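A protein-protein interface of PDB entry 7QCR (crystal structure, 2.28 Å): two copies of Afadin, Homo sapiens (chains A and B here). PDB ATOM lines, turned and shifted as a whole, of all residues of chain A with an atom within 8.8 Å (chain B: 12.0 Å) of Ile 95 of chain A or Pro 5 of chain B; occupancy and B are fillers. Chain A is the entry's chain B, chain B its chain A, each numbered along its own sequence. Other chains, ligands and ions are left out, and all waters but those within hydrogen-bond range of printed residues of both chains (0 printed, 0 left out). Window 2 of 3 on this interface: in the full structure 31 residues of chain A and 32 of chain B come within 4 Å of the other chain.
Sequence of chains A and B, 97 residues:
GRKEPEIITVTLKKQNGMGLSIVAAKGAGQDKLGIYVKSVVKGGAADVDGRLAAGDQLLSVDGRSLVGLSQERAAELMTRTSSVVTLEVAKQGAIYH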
ATOM      1  N   TYR A  36      -7.058  37.419 -14.970  1.00  0.00           N
ATOM      2  CA  TYR A  36      -6.482  36.684 -13.870  1.00  0.00           C
ATOM      3  C   TYR A  36      -6.059  37.585 -12.712  1.00  0.00           C
ATOM      4  O   TYR A  36      -5.761  38.758 -12.904  1.00  0.00           O
ATOM      5  CB  TYR A  36      -5.290  35.864 -14.388  1.00  0.00           C
ATOM      6  CG  TYR A  36      -5.692  34.873 -15.460  1.00  0.00           C
ATOM      7  CD1 TYR A  36      -6.090  33.587 -15.129  1.00  0.00           C
ATOM      8  CD2 TYR A  36      -5.684  35.227 -16.803  1.00  0.00           C
ATOM      9  CE1 TYR A  36      -6.471  32.680 -16.106  1.00  0.00           C
ATOM     10  CE2 TYR A  36      -6.089  34.336 -17.787  1.00  0.00           C
ATOM     11  CZ  TYR A  36      -6.487  33.065 -17.435  1.00  0.00           C
ATOM     12  OH  TYR A  36      -6.865  32.193 -18.428  1.00  0.00           O
ATOM     13  N   GLY A  55      -3.546  33.881  -9.400  1.00  0.00           N
ATOM     14  CA  GLY A  55      -3.678  32.760 -10.320  1.00  0.00           C
ATOM     15  C   GLY A  55      -5.113  32.391 -10.645  1.00  0.00           C
ATOM     16  O   GLY A  55      -5.363  31.644 -11.598  1.00  0.00           O
ATOM     17  N   ASP A  56      -6.071  32.876  -9.844  1.00  0.00           N
ATOM     18  CA  ASP A  56      -7.487  32.596 -10.090  1.00  0.00           C
ATOM     19  C   ASP A  56      -7.966  33.415 -11.274  1.00  0.00           C
ATOM     20  O   ASP A  56      -7.470  34.523 -11.507  1.00  0.00           O
ATOM     21  CB  ASP A  56      -8.344  32.917  -8.847  1.00  0.00           C
ATOM     22  CG  ASP A  56      -8.097  32.013  -7.659  1.00  0.00           C
ATOM     23  OD1 ASP A  56      -7.404  30.989  -7.823  1.00  0.00           O
ATOM     24  OD2 ASP A  56      -8.592  32.332  -6.563  1.00  0.00           O
ATOM     25  N   GLN A  57      -8.916  32.873 -12.033  1.00  0.00           N
ATOM     26  CA  GLN A  57      -9.452  33.586 -13.179  1.00  0.00           C
ATOM     27  C   GLN A  57     -10.789  34.178 -12.818  1.00  0.00           C
ATOM     28  O   GLN A  57     -11.632  33.484 -12.261  1.00  0.00           O
ATOM     29  CB  GLN A  57      -9.602  32.653 -14.380  1.00  0.00           C
ATOM     30  CG  GLN A  57     -10.093  33.378 -15.627  1.00  0.00           C
ATOM     31  CD  GLN A  57     -10.284  32.475 -16.821  1.00  0.00           C
ATOM     32  OE1 GLN A  57     -10.051  31.262 -16.767  1.00  0.00           O
ATOM     33  NE2 GLN A  57     -10.734  33.053 -17.933  1.00  0.00           N
ATOM     34  N   LEU A  59     -14.064  35.043 -14.092  1.00  0.00           N
ATOM     35  CA  LEU A  59     -14.874  34.692 -15.256  1.00  0.00           C
ATOM     36  C   LEU A  59     -15.955  35.705 -15.580  1.00  0.00           C
ATOM     37  O   LEU A  59     -16.316  35.841 -16.747  1.00  0.00           O
ATOM     38  CB  LEU A  59     -15.481  33.296 -15.099  1.00  0.00           C
ATOM     39  CG  LEU A  59     -14.483  32.209 -14.779  1.00  0.00           C
ATOM     40  CD1 LEU A  59     -15.189  30.954 -14.301  1.00  0.00           C
ATOM     41  CD2 LEU A  59     -13.591  31.951 -15.970  1.00  0.00           C
ATOM     42  N   VAL A  89     -15.594  32.835 -10.150  1.00  0.00           N
ATOM     43  CA  VAL A  89     -14.147  32.613 -10.130  1.00  0.00           C
ATOM     44  C   VAL A  89     -13.758  31.175 -10.465  1.00  0.00           C
ATOM     45  O   VAL A  89     -14.359  30.247  -9.948  1.00  0.00           O
ATOM     46  CB  VAL A  89     -13.583  33.041  -8.732  1.00  0.00           C
ATOM     47  CG1 VAL A  89     -12.087  32.769  -8.601  1.00  0.00           C
ATOM     48  CG2 VAL A  89     -13.899  34.508  -8.426  1.00  0.00           C
ATOM     49  N   ALA A  90     -12.742  30.989 -11.310  1.00  0.00           N
ATOM     50  CA  ALA A  90     -12.216  29.666 -11.606  1.00  0.00           C
ATOM     51  C   ALA A  90     -10.929  29.586 -10.811  1.00  0.00           C
ATOM     52  O   ALA A  90      -9.993  30.330 -11.098  1.00  0.00           O
ATOM     53  CB  ALA A  90     -11.930  29.523 -13.091  1.00  0.00           C
ATOM     54  N   LYS A  91     -10.910  28.760  -9.758  1.00  0.00           N
ATOM     55  CA  LYS A  91      -9.757  28.607  -8.872  1.00  0.00           C
ATOM     56  C   LYS A  91      -8.581  28.064  -9.654  1.00  0.00           C
ATOM     57  O   LYS A  91      -8.694  27.013 -10.276  1.00  0.00           O
ATOM     58  CB  LYS A  91     -10.093  27.703  -7.676  1.00  0.00           C
ATOM     59  CG  LYS A  91     -11.192  28.258  -6.779  1.00  0.00           C
ATOM     60  CD  LYS A  91     -10.755  29.518  -6.058  1.00  0.00           C
ATOM     61  CE  LYS A  91      -9.614  29.268  -5.095  1.00  0.00           C
ATOM     62  NZ  LYS A  91      -9.025  30.534  -4.572  1.00  0.00           N
ATOM     63  N   GLN A  92      -7.476  28.816  -9.668  1.00  0.00           N
ATOM     64  CA  GLN A  92      -6.268  28.532 -10.437  1.00  0.00           C
ATOM     65  C   GLN A  92      -6.578  28.264 -11.901  1.00  0.00           C
ATOM     66  O   GLN A  92      -6.328  27.161 -12.381  1.00  0.00           O
ATOM     67  CB  GLN A  92      -5.410  27.424  -9.806  1.00  0.00           C
ATOM     68  CG  GLN A  92      -4.741  27.824  -8.495  1.00  0.00           C
ATOM     69  CD  GLN A  92      -3.921  29.097  -8.589  1.00  0.00           C
ATOM     70  OE1 GLN A  92      -3.304  29.404  -9.620  1.00  0.00           O
ATOM     71  NE2 GLN A  92      -3.903  29.862  -7.512  1.00  0.00           N
ATOM     72  N   GLY A  93      -7.143  29.286 -12.553  1.00  0.00           N
ATOM     73  CA  GLY A  93      -7.578  29.349 -13.943  1.00  0.00           C
ATOM     74  C   GLY A  93      -6.728  28.721 -15.033  1.00  0.00           C
ATOM     75  O   GLY A  93      -7.224  28.522 -16.140  1.00  0.00           O
ATOM     76  N   ALA A  94      -5.463  28.361 -14.747  1.00  0.00           N
ATOM     77  CA  ALA A  94      -4.587  27.619 -15.676  1.00  0.00           C
ATOM     78  C   ALA A  94      -4.940  26.082 -15.683  1.00  0.00           C
ATOM     79  O   ALA A  94      -4.041  25.228 -15.607  1.00  0.00           O
ATOM     80  CB  ALA A  94      -3.135  27.809 -15.268  1.00  0.00           C
ATOM     81  N   ILE A  95      -6.270  25.763 -15.744  1.00  0.00           N
ATOM     82  CA  ILE A  95      -6.924  24.439 -15.750  1.00  0.00           C
ATOM     83  C   ILE A  95      -6.707  23.693 -14.389  1.00  0.00           C
ATOM     84  O   ILE A  95      -7.088  24.255 -13.336  1.00  0.00           O
ATOM     85  CB  ILE A  95      -6.549  23.605 -17.019  1.00  0.00           C
ATOM     86  CG1 ILE A  95      -6.772  24.437 -18.317  1.00  0.00           C
ATOM     87  CG2 ILE A  95      -7.299  22.253 -17.096  1.00  0.00           C
ATOM     88  CD1 ILE A  95      -8.255  24.600 -18.781  1.00  0.00           C
ATOM     89  N   PRO B   5     -11.070  23.173 -13.449  1.00  0.00           N
ATOM     90  CA  PRO B   5     -10.872  23.846 -12.159  1.00  0.00           C
ATOM     91  C   PRO B   5     -12.144  23.965 -11.319  1.00  0.00           C
ATOM     92  O   PRO B   5     -13.248  23.768 -11.823  1.00  0.00           O
ATOM     93  CB  PRO B   5     -10.341  25.232 -12.561  1.00  0.00           C
ATOM     94  CG  PRO B   5     -10.746  25.408 -13.985  1.00  0.00           C
ATOM     95  CD  PRO B   5     -10.681  24.036 -14.578  1.00  0.00           C
ATOM     96  N   GLU B   6     -11.984  24.309 -10.033  1.00  0.00           N
ATOM     97  CA  GLU B   6     -13.105  24.523  -9.121  1.00  0.00           C
ATOM     98  C   GLU B   6     -13.706  25.892  -9.440  1.00  0.00           C
ATOM     99  O   GLU B   6     -12.968  26.865  -9.500  1.00  0.00           O
ATOM    100  CB  GLU B   6     -12.617  24.496  -7.657  1.00  0.00           C
ATOM    101  CG  GLU B   6     -13.730  24.634  -6.631  1.00  0.00           C
ATOM    102  CD  GLU B   6     -13.284  24.845  -5.195  1.00  0.00           C
ATOM    103  OE1 GLU B   6     -12.082  25.116  -4.971  1.00  0.00           O
ATOM    104  OE2 GLU B   6     -14.145  24.753  -4.290  1.00  0.00           O
ATOM    105  N   ILE B   7     -15.017  25.973  -9.687  1.00  0.00           N
ATOM    106  CA  ILE B   7     -15.659  27.259  -9.981  1.00  0.00           C
ATOM    107  C   ILE B   7     -16.560  27.694  -8.832  1.00  0.00           C
ATOM    108  O   ILE B   7     -17.576  27.052  -8.561  1.00  0.00           O
ATOM    109  CB  ILE B   7     -16.376  27.282 -11.351  1.00  0.00           C
ATOM    110  CG1 ILE B   7     -15.351  27.073 -12.482  1.00  0.00           C
ATOM    111  CG2 ILE B   7     -17.151  28.593 -11.530  1.00  0.00           C
ATOM    112  CD1 ILE B   7     -15.921  27.031 -13.859  1.00  0.00           C
ATOM    113  N   ILE B   8     -16.174  28.776  -8.151  1.00  0.00           N
ATOM    114  CA  ILE B   8     -16.898  29.302  -7.001  1.00  0.00           C
ATOM    115  C   ILE B   8     -17.491  30.691  -7.294  1.00  0.00           C
ATOM    116  O   ILE B   8     -17.098  31.344  -8.259  1.00  0.00           O
ATOM    117  CB  ILE B   8     -15.932  29.327  -5.789  1.00  0.00           C
ATOM    118  CG1 ILE B   8     -16.679  29.264  -4.445  1.00  0.00           C
ATOM    119  CG2 ILE B   8     -14.967  30.507  -5.857  1.00  0.00           C
ATOM    120  CD1 ILE B   8     -15.786  28.864  -3.221  1.00  0.00           C
ATOM    121  N   THR B   9     -18.457  31.142  -6.479  1.00  0.00           N
ATOM    122  CA  THR B   9     -19.071  32.452  -6.652  1.00  0.00           C
ATOM    123  C   THR B   9     -18.741  33.288  -5.427  1.00  0.00           C
ATOM    124  O   THR B   9     -19.117  32.935  -4.313  1.00  0.00           O
ATOM    125  CB  THR B   9     -20.571  32.329  -6.943  1.00  0.00           C
ATOM    126  OG1 THR B   9     -20.743  31.856  -8.283  1.00  0.00           O
ATOM    127  CG2 THR B   9     -21.298  33.649  -6.800  1.00  0.00           C
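N of Lys 91 of chain A lies within hydrogen-bond range of O of Glu 6 of chain B (2.8 Å). The backbone carbonyl oxygen of Ile 8 of chain B sits at hydrogen-bond distance from the backbone NH of Val 89 of chain A (2.8 Å).
NZ of Lys 91 of chain A lies within salt-bridge range of OD2 of Asp 56 of chain A (2.7 Å). The backbone carbonyl oxygen of Gln 57 of chain A sits at hydrogen-bond distance from the backbone NH of Ala 90 of chain A, 2.9 Å away.
Among the printed residues, pairs that only touch across the chains: Val 89 of chain A with Glu 6 of chain B, Val 89 of chain A with Ile 7 of chain B, Ala 90 of chain A with Glu 6 of chain B, Lys 91 of chain A with Pro 5 of chain B and Ile 95 of chain A with Pro 5 of chain B.
Of chain A, only Lys 91 (3.3 Å) and Ile 95 (3.5 Å) come within 4 Å of Pro 5 of chain B. Ala 90 of chain A touches just one residue of chain B: Glu 6. No residue of chain B comes within 4 Å of Gly 93 of chain A. Printed residues of chain A within 4 Å of Glu 6 of chain B: Val 89 (3.7 Å), Ala 90 (3.6 Å) and Lys 91 (2.8 Å). Of the printed residues of chain A, Ile 8 of chain B touches Val 89. Of the printed residues of chain B, Val 89 of chain A touches Glu 6, Ile 7 and Ile 8. Of the printed residues of chain B, Lys 91 of chain A touches Pro 5 and Glu 6. Of the printed residues of chain A, Ile 7 of chain B touches Val 89. Asp 56 of chain A touches none of the printed residues of chain B. Leu 59 of chain A touches none of the printed residues of chain B. The nearest residue of chain B that does not touch Ile 95 of chain A is Glu 6 of chain B (5.9 Å). The nearest residue of chain A that does not touch Pro 5 of chain B is Ala 90 of chain A (4.4 Å). The nearest printed residue of chain A that does not touch Ile 8 of chain B is Lys 91 of chain A (4.3 Å).
Of the 12 printed residues of chain A, 4 touch a printed residue of chain B. Of the 5 printed residues of chain B, 4 touch a printed residue of chain A. Printed residues of chain B that touch a printed residue of chain A: Pro 5, Glu 6, Ile 7 and Ile 8. Hydrophobic or aromatic side chains of chain B that line the printed part of chain A: Pro 5 and Ile 7. Along chain B the printed residues that touch a printed residue of chain A span positions 5 to 8. Among the printed residues, no Asp or Glu carboxylate lies within 4 Å of a Lys or Arg side-chain nitrogen of the other chain.
No position is printed for both chains.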
